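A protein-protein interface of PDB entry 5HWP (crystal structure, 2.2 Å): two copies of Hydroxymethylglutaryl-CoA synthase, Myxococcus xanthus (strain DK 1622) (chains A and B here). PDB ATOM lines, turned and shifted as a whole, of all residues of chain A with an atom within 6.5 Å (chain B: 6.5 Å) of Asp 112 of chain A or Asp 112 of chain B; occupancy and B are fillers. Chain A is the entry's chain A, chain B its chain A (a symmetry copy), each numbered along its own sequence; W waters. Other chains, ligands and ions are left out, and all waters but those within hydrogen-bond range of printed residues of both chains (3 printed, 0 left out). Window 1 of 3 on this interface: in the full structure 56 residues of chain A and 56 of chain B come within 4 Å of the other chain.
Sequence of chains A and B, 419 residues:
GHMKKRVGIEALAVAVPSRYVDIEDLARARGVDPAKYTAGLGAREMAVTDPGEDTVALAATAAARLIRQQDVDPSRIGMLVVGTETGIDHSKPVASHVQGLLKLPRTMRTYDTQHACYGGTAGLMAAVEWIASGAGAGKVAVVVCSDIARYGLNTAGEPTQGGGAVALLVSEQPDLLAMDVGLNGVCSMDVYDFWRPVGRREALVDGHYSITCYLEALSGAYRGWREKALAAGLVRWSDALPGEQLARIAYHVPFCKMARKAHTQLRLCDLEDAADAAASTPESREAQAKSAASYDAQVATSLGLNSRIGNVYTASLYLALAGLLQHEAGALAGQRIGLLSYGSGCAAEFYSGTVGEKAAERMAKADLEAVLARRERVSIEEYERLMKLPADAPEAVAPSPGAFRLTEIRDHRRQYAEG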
ATOM      1  N   LEU A  80     -10.098  -5.825  -3.468  1.00  0.00           N
ATOM      2  CA  LEU A  80      -9.586  -6.104  -4.806  1.00  0.00           C
ATOM      3  C   LEU A  80      -9.945  -7.543  -5.142  1.00  0.00           C
ATOM      4  O   LEU A  80      -9.382  -8.478  -4.564  1.00  0.00           O
ATOM      5  CB  LEU A  80      -8.075  -5.886  -4.886  1.00  0.00           C
ATOM      6  CG  LEU A  80      -7.410  -6.355  -6.185  1.00  0.00           C
ATOM      7  CD1 LEU A  80      -7.958  -5.597  -7.388  1.00  0.00           C
ATOM      8  CD2 LEU A  80      -5.899  -6.208  -6.099  1.00  0.00           C
ATOM      9  N   VAL A  81     -10.878  -7.722  -6.072  1.00  0.00           N
ATOM     10  CA  VAL A  81     -11.369  -9.041  -6.447  1.00  0.00           C
ATOM     11  C   VAL A  81     -11.156  -9.233  -7.941  1.00  0.00           C
ATOM     12  O   VAL A  81     -11.386  -8.314  -8.735  1.00  0.00           O
ATOM     13  CB  VAL A  81     -12.857  -9.215  -6.074  1.00  0.00           C
ATOM     14  CG1 VAL A  81     -13.357 -10.600  -6.467  1.00  0.00           C
ATOM     15  CG2 VAL A  81     -13.055  -8.980  -4.584  1.00  0.00           C
ATOM     16  N   VAL A  82     -10.717 -10.431  -8.320  1.00  0.00           N
ATOM     17  CA  VAL A  82     -10.509 -10.790  -9.718  1.00  0.00           C
ATOM     18  C   VAL A  82     -11.490 -11.905 -10.054  1.00  0.00           C
ATOM     19  O   VAL A  82     -11.388 -13.014  -9.514  1.00  0.00           O
ATOM     20  CB  VAL A  82      -9.063 -11.225 -10.002  1.00  0.00           C
ATOM     21  CG1 VAL A  82      -8.929 -11.745 -11.433  1.00  0.00           C
ATOM     22  CG2 VAL A  82      -8.102 -10.067  -9.768  1.00  0.00           C
ATOM     23  N   GLY A  83     -12.441 -11.612 -10.939  1.00  0.00           N
ATOM     24  CA  GLY A  83     -13.275 -12.657 -11.509  1.00  0.00           C
ATOM     25  C   GLY A  83     -12.583 -13.263 -12.711  1.00  0.00           C
ATOM     26  O   GLY A  83     -12.179 -12.551 -13.635  1.00  0.00           O
ATOM     27  N   THR A  84     -12.434 -14.585 -12.696  1.00  0.00           N
ATOM     28  CA  THR A  84     -11.716 -15.265 -13.764  1.00  0.00           C
ATOM     29  C   THR A  84     -12.072 -16.742 -13.760  1.00  0.00           C
ATOM     30  O   THR A  84     -12.318 -17.334 -12.706  1.00  0.00           O
ATOM     31  CB  THR A  84     -10.197 -15.102 -13.612  1.00  0.00           C
ATOM     32  OG1 THR A  84      -9.532 -15.634 -14.766  1.00  0.00           O
ATOM     33  CG2 THR A  84      -9.684 -15.818 -12.356  1.00  0.00           C
ATOM     34  N   GLY A  87      -7.638 -19.212 -13.951  1.00  0.00           N
ATOM     35  CA  GLY A  87      -6.732 -19.110 -12.826  1.00  0.00           C
ATOM     36  C   GLY A  87      -5.389 -19.749 -13.124  1.00  0.00           C
ATOM     37  O   GLY A  87      -5.266 -20.634 -13.968  1.00  0.00           O
ATOM     38  N   ILE A  88      -4.365 -19.301 -12.394  1.00  0.00           N
ATOM     39  CA  ILE A  88      -2.997 -19.759 -12.591  1.00  0.00           C
ATOM     40  C   ILE A  88      -2.447 -20.459 -11.355  1.00  0.00           C
ATOM     41  O   ILE A  88      -1.278 -20.839 -11.332  1.00  0.00           O
ATOM     42  CB  ILE A  88      -2.074 -18.600 -13.024  1.00  0.00           C
ATOM     43  CG1 ILE A  88      -2.228 -17.376 -12.113  1.00  0.00           C
ATOM     44  CG2 ILE A  88      -2.353 -18.221 -14.466  1.00  0.00           C
ATOM     45  CD1 ILE A  88      -1.546 -17.490 -10.760  1.00  0.00           C
ATOM     46  N   ASP A  89      -3.272 -20.647 -10.327  1.00  0.00           N
ATOM     47  CA  ASP A  89      -2.852 -21.363  -9.131  1.00  0.00           C
ATOM     48  C   ASP A  89      -4.087 -21.875  -8.408  1.00  0.00           C
ATOM     49  O   ASP A  89      -5.115 -21.192  -8.372  1.00  0.00           O
ATOM     50  CB  ASP A  89      -2.027 -20.464  -8.202  1.00  0.00           C
ATOM     51  CG  ASP A  89      -1.204 -21.255  -7.206  1.00  0.00           C
ATOM     52  OD1 ASP A  89      -0.060 -21.630  -7.544  1.00  0.00           O
ATOM     53  OD2 ASP A  89      -1.696 -21.499  -6.086  1.00  0.00           O
ATOM     54  N   LYS A  92      -3.031 -19.535  -4.701  1.00  0.00           N
ATOM     55  CA  LYS A  92      -2.707 -18.114  -4.739  1.00  0.00           C
ATOM     56  C   LYS A  92      -3.576 -17.415  -5.779  1.00  0.00           C
ATOM     57  O   LYS A  92      -3.536 -17.793  -6.955  1.00  0.00           O
ATOM     58  CB  LYS A  92      -1.232 -17.921  -5.062  1.00  0.00           C
ATOM     59  CG  LYS A  92      -0.761 -16.477  -5.029  1.00  0.00           C
ATOM     60  CD  LYS A  92       0.753 -16.404  -5.137  1.00  0.00           C
ATOM     61  CE  LYS A  92       1.242 -14.970  -5.289  1.00  0.00           C
ATOM     62  NZ  LYS A  92       0.954 -14.143  -4.086  1.00  0.00           N
ATOM     63  N   PRO A  93      -4.367 -16.412  -5.404  1.00  0.00           N
ATOM     64  CA  PRO A  93      -5.275 -15.792  -6.372  1.00  0.00           C
ATOM     65  C   PRO A  93      -4.579 -14.768  -7.252  1.00  0.00           C
ATOM     66  O   PRO A  93      -3.559 -14.176  -6.886  1.00  0.00           O
ATOM     67  CB  PRO A  93      -6.323 -15.119  -5.479  1.00  0.00           C
ATOM     68  CG  PRO A  93      -5.550 -14.730  -4.273  1.00  0.00           C
ATOM     69  CD  PRO A  93      -4.529 -15.825  -4.061  1.00  0.00           C
ATOM     70  N   VAL A  94      -5.156 -14.564  -8.439  1.00  0.00           N
ATOM     71  CA  VAL A  94      -4.678 -13.515  -9.334  1.00  0.00           C
ATOM     72  C   VAL A  94      -4.698 -12.168  -8.625  1.00  0.00           C
ATOM     73  O   VAL A  94      -3.821 -11.322  -8.836  1.00  0.00           O
ATOM     74  CB  VAL A  94      -5.525 -13.491 -10.622  1.00  0.00           C
ATOM     75  CG1 VAL A  94      -5.169 -12.292 -11.498  1.00  0.00           C
ATOM     76  CG2 VAL A  94      -5.340 -14.785 -11.399  1.00  0.00           C
ATOM     77  N   ALA A  95      -5.698 -11.949  -7.769  1.00  0.00           N
ATOM     78  CA  ALA A  95      -5.807 -10.680  -7.057  1.00  0.00           C
ATOM     79  C   ALA A  95      -4.547 -10.379  -6.255  1.00  0.00           C
ATOM     80  O   ALA A  95      -4.114  -9.223  -6.176  1.00  0.00           O
ATOM     81  CB  ALA A  95      -7.030 -10.697  -6.139  1.00  0.00           C
ATOM     82  N   SER A  96      -3.943 -11.402  -5.645  1.00  0.00           N
ATOM     83  CA  SER A  96      -2.732 -11.172  -4.862  1.00  0.00           C
ATOM     84  C   SER A  96      -1.564 -10.794  -5.762  1.00  0.00           C
ATOM     85  O   SER A  96      -0.749  -9.938  -5.400  1.00  0.00           O
ATOM     86  CB  SER A  96      -2.394 -12.408  -4.029  1.00  0.00           C
ATOM     87  OG  SER A  96      -1.873 -13.447  -4.837  1.00  0.00           O
ATOM     88  N   THR A 110      -8.362  -9.326  -0.639  1.00  0.00           N
ATOM     89  CA  THR A 110      -8.022  -9.811  -1.966  1.00  0.00           C
ATOM     90  C   THR A 110      -8.506 -11.246  -2.089  1.00  0.00           C
ATOM     91  O   THR A 110      -8.415 -12.020  -1.133  1.00  0.00           O
ATOM     92  CB  THR A 110      -6.506  -9.719  -2.236  1.00  0.00           C
ATOM     93  OG1 THR A 110      -5.794 -10.561  -1.322  1.00  0.00           O
ATOM     94  CG2 THR A 110      -6.021  -8.288  -2.068  1.00  0.00           C
ATOM     95  N   TYR A 111      -9.070 -11.579  -3.246  1.00  0.00           N
ATOM     96  CA  TYR A 111      -9.419 -12.960  -3.557  1.00  0.00           C
ATOM     97  C   TYR A 111      -9.944 -13.016  -4.983  1.00  0.00           C
ATOM     98  O   TYR A 111     -10.173 -11.988  -5.624  1.00  0.00           O
ATOM     99  CB  TYR A 111     -10.446 -13.539  -2.572  1.00  0.00           C
ATOM    100  CG  TYR A 111     -11.781 -12.821  -2.505  1.00  0.00           C
ATOM    101  CD1 TYR A 111     -12.829 -13.183  -3.344  1.00  0.00           C
ATOM    102  CD2 TYR A 111     -12.008 -11.810  -1.577  1.00  0.00           C
ATOM    103  CE1 TYR A 111     -14.055 -12.546  -3.278  1.00  0.00           C
ATOM    104  CE2 TYR A 111     -13.233 -11.169  -1.504  1.00  0.00           C
ATOM    105  CZ  TYR A 111     -14.253 -11.541  -2.357  1.00  0.00           C
ATOM    106  OH  TYR A 111     -15.472 -10.907  -2.285  1.00  0.00           O
ATOM    107  N   ASP A 112     -10.114 -14.238  -5.475  1.00  0.00           N
ATOM    108  CA  ASP A 112     -10.680 -14.487  -6.790  1.00  0.00           C
ATOM    109  C   ASP A 112     -12.059 -15.117  -6.649  1.00  0.00           C
ATOM    110  O   ASP A 112     -12.322 -15.869  -5.708  1.00  0.00           O
ATOM    111  CB  ASP A 112      -9.778 -15.410  -7.617  1.00  0.00           C
ATOM    112  CG  ASP A 112      -8.456 -14.761  -7.981  1.00  0.00           C
ATOM    113  OD1 ASP A 112      -8.295 -13.548  -7.734  1.00  0.00           O
ATOM    114  OD2 ASP A 112      -7.581 -15.464  -8.526  1.00  0.00           O
ATOM    115  N   THR A 113     -12.936 -14.797  -7.596  1.00  0.00           N
ATOM    116  CA  THR A 113     -14.250 -15.410  -7.697  1.00  0.00           C
ATOM    117  C   THR A 113     -14.320 -16.227  -8.980  1.00  0.00           C
ATOM    118  O   THR A 113     -13.801 -15.806 -10.019  1.00  0.00           O
ATOM    119  CB  THR A 113     -15.358 -14.355  -7.689  1.00  0.00           C
ATOM    120  OG1 THR A 113     -15.037 -13.315  -8.622  1.00  0.00           O
ATOM    121  CG2 THR A 113     -15.526 -13.756  -6.297  1.00  0.00           C
ATOM    122  N   GLN A 114     -14.952 -17.398  -8.908  1.00  0.00           N
ATOM    123  CA  GLN A 114     -15.029 -18.298 -10.054  1.00  0.00           C
ATOM    124  C   GLN A 114     -16.460 -18.766 -10.270  1.00  0.00           C
ATOM    125  O   GLN A 114     -17.072 -19.350  -9.369  1.00  0.00           O
ATOM    126  CB  GLN A 114     -14.112 -19.515  -9.879  1.00  0.00           C
ATOM    127  CG  GLN A 114     -14.140 -20.462 -11.083  1.00  0.00           C
ATOM    128  CD  GLN A 114     -13.538 -21.820 -10.789  1.00  0.00           C
ATOM    129  OE1 GLN A 114     -14.131 -22.852 -11.101  1.00  0.00           O
ATOM    130  NE2 GLN A 114     -12.354 -21.829 -10.195  1.00  0.00           N
ATOM    131  N   HIS A 115     -16.981 -18.505 -11.468  1.00  0.00           N
ATOM    132  CA  HIS A 115     -18.090 -19.259 -12.038  1.00  0.00           C
ATOM    133  C   HIS A 115     -18.176 -18.950 -13.526  1.00  0.00           C
ATOM    134  O   HIS A 115     -19.005 -18.138 -13.951  1.00  0.00           O
ATOM    135  CB  HIS A 115     -19.422 -18.944 -11.356  1.00  0.00           C
ATOM    136  CG  HIS A 115     -20.532 -19.864 -11.763  1.00  0.00           C
ATOM    137  ND1 HIS A 115     -20.489 -20.614 -12.919  1.00  0.00           N
ATOM    138  CD2 HIS A 115     -21.703 -20.173 -11.160  1.00  0.00           C
ATOM    139  CE1 HIS A 115     -21.591 -21.337 -13.014  1.00  0.00           C
ATOM    140  NE2 HIS A 115     -22.345 -21.088 -11.960  1.00  0.00           N
ATOM    141  N   LEU B  80     -25.188 -19.486  -2.566  1.00  0.00           N
ATOM    142  CA  LEU B  80     -24.424 -20.684  -2.237  1.00  0.00           C
ATOM    143  C   LEU B  80     -23.004 -20.472  -2.738  1.00  0.00           C
ATOM    144  O   LEU B  80     -22.765 -20.466  -3.950  1.00  0.00           O
ATOM    145  CB  LEU B  80     -25.042 -21.935  -2.861  1.00  0.00           C
ATOM    146  CG  LEU B  80     -24.199 -23.211  -2.754  1.00  0.00           C
ATOM    147  CD1 LEU B  80     -23.971 -23.598  -1.298  1.00  0.00           C
ATOM    148  CD2 LEU B  80     -24.850 -24.352  -3.518  1.00  0.00           C
ATOM    149  N   VAL B  81     -22.065 -20.301  -1.813  1.00  0.00           N
ATOM    150  CA  VAL B  81     -20.675 -20.021  -2.148  1.00  0.00           C
ATOM    151  C   VAL B  81     -19.797 -21.091  -1.515  1.00  0.00           C
ATOM    152  O   VAL B  81     -20.018 -21.489  -0.366  1.00  0.00           O
ATOM    153  CB  VAL B  81     -20.255 -18.612  -1.677  1.00  0.00           C
ATOM    154  CG1 VAL B  81     -18.801 -18.330  -2.038  1.00  0.00           C
ATOM    155  CG2 VAL B  81     -21.169 -17.560  -2.289  1.00  0.00           C
ATOM    156  N   VAL B  82     -18.802 -21.552  -2.269  1.00  0.00           N
ATOM    157  CA  VAL B  82     -17.844 -22.542  -1.792  1.00  0.00           C
ATOM    158  C   VAL B  82     -16.476 -21.876  -1.763  1.00  0.00           C
ATOM    159  O   VAL B  82     -15.930 -21.515  -2.814  1.00  0.00           O
ATOM    160  CB  VAL B  82     -17.822 -23.805  -2.667  1.00  0.00           C
ATOM    161  CG1 VAL B  82     -16.697 -24.742  -2.231  1.00  0.00           C
ATOM    162  CG2 VAL B  82     -19.163 -24.523  -2.601  1.00  0.00           C
ATOM    163  N   GLY B  83     -15.923 -21.707  -0.562  1.00  0.00           N
ATOM    164  CA  GLY B  83     -14.532 -21.306  -0.432  1.00  0.00           C
ATOM    165  C   GLY B  83     -13.643 -22.530  -0.480  1.00  0.00           C
ATOM    166  O   GLY B  83     -13.837 -23.484   0.279  1.00  0.00           O
ATOM    167  N   THR B  84     -12.666 -22.510  -1.383  1.00  0.00           N
ATOM    168  CA  THR B  84     -11.799 -23.664  -1.568  1.00  0.00           C
ATOM    169  C   THR B  84     -10.532 -23.241  -2.292  1.00  0.00           C
ATOM    170  O   THR B  84     -10.552 -22.342  -3.135  1.00  0.00           O
ATOM    171  CB  THR B  84     -12.501 -24.773  -2.365  1.00  0.00           C
ATOM    172  OG1 THR B  84     -11.686 -25.952  -2.380  1.00  0.00           O
ATOM    173  CG2 THR B  84     -12.778 -24.329  -3.807  1.00  0.00           C
ATOM    174  N   GLY B  87      -9.941 -26.584  -6.069  1.00  0.00           N
ATOM    175  CA  GLY B  87     -10.915 -26.608  -7.141  1.00  0.00           C
ATOM    176  C   GLY B  87     -10.693 -27.779  -8.079  1.00  0.00           C
ATOM    177  O   GLY B  87      -9.591 -28.311  -8.201  1.00  0.00           O
ATOM    178  N   ILE B  88     -11.765 -28.171  -8.771  1.00  0.00           N
ATOM    179  CA  ILE B  88     -11.746 -29.317  -9.668  1.00  0.00           C
ATOM    180  C   ILE B  88     -12.037 -28.917 -11.109  1.00  0.00           C
ATOM    181  O   ILE B  88     -12.133 -29.779 -11.980  1.00  0.00           O
ATOM    182  CB  ILE B  88     -12.721 -30.417  -9.195  1.00  0.00           C
ATOM    183  CG1 ILE B  88     -14.112 -29.853  -8.885  1.00  0.00           C
ATOM    184  CG2 ILE B  88     -12.157 -31.126  -7.978  1.00  0.00           C
ATOM    185  CD1 ILE B  88     -14.966 -29.540 -10.102  1.00  0.00           C
ATOM    186  N   ASP B  89     -12.171 -27.620 -11.380  1.00  0.00           N
ATOM    187  CA  ASP B  89     -12.386 -27.142 -12.738  1.00  0.00           C
ATOM    188  C   ASP B  89     -11.970 -25.681 -12.813  1.00  0.00           C
ATOM    189  O   ASP B  89     -12.189 -24.922 -11.865  1.00  0.00           O
ATOM    190  CB  ASP B  89     -13.851 -27.299 -13.161  1.00  0.00           C
ATOM    191  CG  ASP B  89     -14.032 -27.251 -14.665  1.00  0.00           C
ATOM    192  OD1 ASP B  89     -13.931 -28.318 -15.310  1.00  0.00           O
ATOM    193  OD2 ASP B  89     -14.279 -26.152 -15.201  1.00  0.00           O
ATOM    194  N   LYS B  92     -16.118 -24.445 -14.079  1.00  0.00           N
ATOM    195  CA  LYS B  92     -17.313 -24.858 -13.353  1.00  0.00           C
ATOM    196  C   LYS B  92     -17.022 -24.889 -11.856  1.00  0.00           C
ATOM    197  O   LYS B  92     -16.113 -25.609 -11.430  1.00  0.00           O
ATOM    198  CB  LYS B  92     -17.770 -26.228 -13.834  1.00  0.00           C
ATOM    199  CG  LYS B  92     -19.068 -26.715 -13.213  1.00  0.00           C
ATOM    200  CD  LYS B  92     -19.560 -27.971 -13.913  1.00  0.00           C
ATOM    201  CE  LYS B  92     -20.758 -28.585 -13.201  1.00  0.00           C
ATOM    202  NZ  LYS B  92     -21.952 -27.698 -13.234  1.00  0.00           N
ATOM    203  N   PRO B  93     -17.748 -24.136 -11.033  1.00  0.00           N
ATOM    204  CA  PRO B  93     -17.422 -24.084  -9.606  1.00  0.00           C
ATOM    205  C   PRO B  93     -17.978 -25.269  -8.836  1.00  0.00           C
ATOM    206  O   PRO B  93     -18.966 -25.897  -9.227  1.00  0.00           O
ATOM    207  CB  PRO B  93     -18.083 -22.779  -9.149  1.00  0.00           C
ATOM    208  CG  PRO B  93     -19.281 -22.676 -10.019  1.00  0.00           C
ATOM    209  CD  PRO B  93     -18.870 -23.237 -11.361  1.00  0.00           C
ATOM    210  N   VAL B  94     -17.317 -25.570  -7.715  1.00  0.00           N
ATOM    211  CA  VAL B  94     -17.814 -26.597  -6.805  1.00  0.00           C
ATOM    212  C   VAL B  94     -19.238 -26.274  -6.374  1.00  0.00           C
ATOM    213  O   VAL B  94     -20.071 -27.171  -6.197  1.00  0.00           O
ATOM    214  CB  VAL B  94     -16.871 -26.732  -5.593  1.00  0.00           C
ATOM    215  CG1 VAL B  94     -17.457 -27.666  -4.536  1.00  0.00           C
ATOM    216  CG2 VAL B  94     -15.506 -27.232  -6.041  1.00  0.00           C
ATOM    217  N   ALA B  95     -19.541 -24.985  -6.201  1.00  0.00           N
ATOM    218  CA  ALA B  95     -20.876 -24.583  -5.772  1.00  0.00           C
ATOM    219  C   ALA B  95     -21.948 -25.102  -6.723  1.00  0.00           C
ATOM    220  O   ALA B  95     -23.034 -25.503  -6.286  1.00  0.00           O
ATOM    221  CB  ALA B  95     -20.955 -23.061  -5.661  1.00  0.00           C
ATOM    222  N   SER B  96     -21.670 -25.099  -8.029  1.00  0.00           N
ATOM    223  CA  SER B  96     -22.661 -25.583  -8.986  1.00  0.00           C
ATOM    224  C   SER B  96     -22.856 -27.088  -8.855  1.00  0.00           C
ATOM    225  O   SER B  96     -23.983 -27.584  -8.970  1.00  0.00           O
ATOM    226  CB  SER B  96     -22.250 -25.215 -10.410  1.00  0.00           C
ATOM    227  OG  SER B  96     -21.176 -26.020 -10.862  1.00  0.00           O
ATOM    228  N   THR B 110     -24.527 -18.759  -7.288  1.00  0.00           N
ATOM    229  CA  THR B 110     -23.551 -19.797  -7.002  1.00  0.00           C
ATOM    230  C   THR B 110     -22.207 -19.356  -7.557  1.00  0.00           C
ATOM    231  O   THR B 110     -22.142 -18.763  -8.637  1.00  0.00           O
ATOM    232  CB  THR B 110     -23.970 -21.156  -7.597  1.00  0.00           C
ATOM    233  OG1 THR B 110     -24.032 -21.067  -9.025  1.00  0.00           O
ATOM    234  CG2 THR B 110     -25.336 -21.569  -7.070  1.00  0.00           C
ATOM    235  N   TYR B 111     -21.147 -19.597  -6.792  1.00  0.00           N
ATOM    236  CA  TYR B 111     -19.788 -19.383  -7.278  1.00  0.00           C
ATOM    237  C   TYR B 111     -18.814 -19.848  -6.208  1.00  0.00           C
ATOM    238  O   TYR B 111     -19.201 -20.164  -5.080  1.00  0.00           O
ATOM    239  CB  TYR B 111     -19.528 -17.917  -7.657  1.00  0.00           C
ATOM    240  CG  TYR B 111     -19.691 -16.902  -6.541  1.00  0.00           C
ATOM    241  CD1 TYR B 111     -18.621 -16.567  -5.721  1.00  0.00           C
ATOM    242  CD2 TYR B 111     -20.902 -16.250  -6.334  1.00  0.00           C
ATOM    243  CE1 TYR B 111     -18.755 -15.630  -4.712  1.00  0.00           C
ATOM    244  CE2 TYR B 111     -21.044 -15.310  -5.328  1.00  0.00           C
ATOM    245  CZ  TYR B 111     -19.967 -15.004  -4.520  1.00  0.00           C
ATOM    246  OH  TYR B 111     -20.105 -14.068  -3.520  1.00  0.00           O
ATOM    247  N   ASP B 112     -17.542 -19.900  -6.585  1.00  0.00           N
ATOM    248  CA  ASP B 112     -16.462 -20.246  -5.677  1.00  0.00           C
ATOM    249  C   ASP B 112     -15.597 -19.021  -5.411  1.00  0.00           C
ATOM    250  O   ASP B 112     -15.426 -18.162  -6.280  1.00  0.00           O
ATOM    251  CB  ASP B 112     -15.594 -21.371  -6.248  1.00  0.00           C
ATOM    252  CG  ASP B 112     -16.335 -22.691  -6.342  1.00  0.00           C
ATOM    253  OD1 ASP B 112     -17.467 -22.782  -5.822  1.00  0.00           O
ATOM    254  OD2 ASP B 112     -15.779 -23.644  -6.927  1.00  0.00           O
ATOM    255  N   THR B 113     -15.058 -18.951  -4.199  1.00  0.00           N
ATOM    256  CA  THR B 113     -14.098 -17.928  -3.817  1.00  0.00           C
ATOM    257  C   THR B 113     -12.753 -18.586  -3.542  1.00  0.00           C
ATOM    258  O   THR B 113     -12.696 -19.673  -2.956  1.00  0.00           O
ATOM    259  CB  THR B 113     -14.566 -17.159  -2.580  1.00  0.00           C
ATOM    260  OG1 THR B 113     -14.986 -18.086  -1.569  1.00  0.00           O
ATOM    261  CG2 THR B 113     -15.722 -16.227  -2.926  1.00  0.00           C
ATOM    262  N   GLN B 114     -11.671 -17.935  -3.968  1.00  0.00           N
ATOM    263  CA  GLN B 114     -10.332 -18.495  -3.819  1.00  0.00           C
ATOM    264  C   GLN B 114      -9.387 -17.465  -3.219  1.00  0.00           C
ATOM    265  O   GLN B 114      -9.212 -16.376  -3.775  1.00  0.00           O
ATOM    266  CB  GLN B 114      -9.773 -18.986  -5.160  1.00  0.00           C
ATOM    267  CG  GLN B 114      -8.382 -19.615  -5.032  1.00  0.00           C
ATOM    268  CD  GLN B 114      -7.673 -19.773  -6.361  1.00  0.00           C
ATOM    269  OE1 GLN B 114      -6.508 -19.403  -6.501  1.00  0.00           O
ATOM    270  NE2 GLN B 114      -8.368 -20.331  -7.343  1.00  0.00           N
ATOM    271  N   HIS B 115      -8.783 -17.823  -2.088  1.00  0.00           N
ATOM    272  CA  HIS B 115      -7.529 -17.235  -1.632  1.00  0.00           C
ATOM    273  C   HIS B 115      -6.950 -18.116  -0.534  1.00  0.00           C
ATOM    274  O   HIS B 115      -7.088 -17.809   0.655  1.00  0.00           O
ATOM    275  CB  HIS B 115      -7.706 -15.804  -1.121  1.00  0.00           C
ATOM    276  CG  HIS B 115      -6.410 -15.100  -0.862  1.00  0.00           C
ATOM    277  ND1 HIS B 115      -5.222 -15.775  -0.678  1.00  0.00           N
ATOM    278  CD2 HIS B 115      -6.110 -13.784  -0.776  1.00  0.00           C
ATOM    279  CE1 HIS B 115      -4.249 -14.903  -0.481  1.00  0.00           C
ATOM    280  NE2 HIS B 115      -4.760 -13.687  -0.536  1.00  0.00           N
HETATM  281  O   HOH W   1      -7.611 -18.155  -9.364  1.00  0.00           O
HETATM  282  O   HOH W   2     -12.431 -18.685  -7.133  1.00  0.00           O
HETATM  283  O   HOH W   3     -13.222 -23.877  -8.086  1.00  0.00           O
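OE1 of Gln 114 of chain B sits close to O of Asp 89 of chain A (2.9 Å).
OE1 of Gln 114 of chain B sits close to O of Lys 92 of chain A.
OG1 of Thr 110 of chain A sits close to NE2 of His 115 of chain B.
The backbone carbonyl oxygen (O) of Asp 112 of chain A lies within hydrogen-bond range of the backbone NH (N) of Gln 114 of chain B.
The side-chain amide oxygen (OE1) of Gln 114 of chain A sits close to the backbone carbonyl oxygen (O) of Asp 89 of chain B (2.9 Å).
OE1 of Gln 114 of chain A sits close to O of Lys 92 of chain B (3.4 Å).
N of Gln 114 of chain A lies within hydrogen-bond range of O of Asp 112 of chain B.
NE2 of His 115 of chain A lies close to OG1 of Thr 110 of chain B (3.4 Å).
O of Tyr 111 of chain A sits at hydrogen-bond distance from N of Val 82 of chain A (3.2 Å).
The side-chain amino group of Lys 92 of chain A is in hydrogen-bond range of the side-chain hydroxyl of Ser 96 of chain A.
N of Val 94 of chain A sits at hydrogen-bond distance from OD2 of Asp 112 of chain A (2.6 Å).
The backbone NH (N) of Val 82 of chain B is in hydrogen-bond range of the backbone carbonyl oxygen (O) of Tyr 111 of chain B, at 3.2 Å.
O of Pro 93 of chain B sits at hydrogen-bond distance from OG of Ser 96 of chain B, 2.8 Å away.
OD2 of Asp 112 of chain B lies within hydrogen-bond range of N of Val 94 of chain B, 2.6 Å away.
His 115 of chain B touches Pro 93 of chain A.
CB of Tyr 111 of chain A touches O of Gln 114 of chain B (3.3 Å).
Tyr 111 of chain A touches His 115 of chain B.
Asp 112 of chain B touches Asp 112 of chain A.
CA of Thr 113 of chain B touches O of Asp 112 of chain A (3.3 Å).
Thr 113 of chain A touches Asp 112 of chain B.
O of Gln 114 of chain A touches CB of Pro 93 of chain B, at 3.6 Å.
Tyr 111 of chain B touches Gln 114 of chain A (CB to O, 3.3 Å).
His 115 of chain A touches Pro 93 of chain B (ND1 to CD, 3.5 Å).
CB of Tyr 111 of chain B touches CB of His 115 of chain A, 3.8 Å away.
Asp 112 of chain A touches just these residues of chain B: Asp 112 (3.9 Å), Thr 113 (3.3 Å) and Gln 114 (2.8 Å).
Asp 112 of chain B touches three residues of chain A.
Of the printed residues of chain A, Asp 89 of chain B touches Gln 114 (2.9 Å).
Printed residues of chain B within 4 Å of Thr 110 of chain A: His 115 (2.9 Å).
The nearest residue of chain A that does not touch Asp 112 of chain B is His 115 of chain A (5.1 Å).
Of the 19 printed residues of chain A, 9 touch a printed residue of chain B.
Printed residues of chain A that touch a printed residue of chain B: Asp 89, Lys 92, Pro 93, Thr 110, Tyr 111, Asp 112, Thr 113, Gln 114 and His 115.
Hydrophobic or aromatic side chains of chain B that line the printed part of chain A: Pro 93, Tyr 111 and His 115.
Among the printed residues, 19 pairs touch across the chains.
Pro 93 of chain A touches Gln 114 of chain B, and with the chains exchanged Gln 114 of chain A touches Pro 93 of chain B.
Tyr 111 of chain A touches Gln 114 of chain B, and with the chains exchanged Gln 114 of chain A touches Tyr 111 of chain B.
Asp 112 of chain B touches its own counterpart, Asp 112 of chain A.
Asp 112 of chain A touches Gln 114 of chain B, and with the chains exchanged Gln 114 of chain A touches Asp 112 of chain B.
19 positions are printed for both chains.
Of the 19 pairs that touch across the chains among the printed residues, 19 have their exchanged pair printed and touching as well.
Water W1 lies within hydrogen-bond range of OD2 of Asp 112 of chain A and NE2 of Gln 114 of chain B.
Water W3 lies within hydrogen-bond range of OD2 of Asp 112 of chain B and NE2 of Gln 114 of chain A.
Water W2 lies within hydrogen-bond range of the backbone carbonyl oxygen of Asp 112 of chain A (3.2 Å), the backbone carbonyl oxygen of Asp 112 of chain B (3.2 Å), the backbone NH of Gln 114 of chain B (3.3 Å) and the backbone NH of Gln 114 of chain A (3.3 Å).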
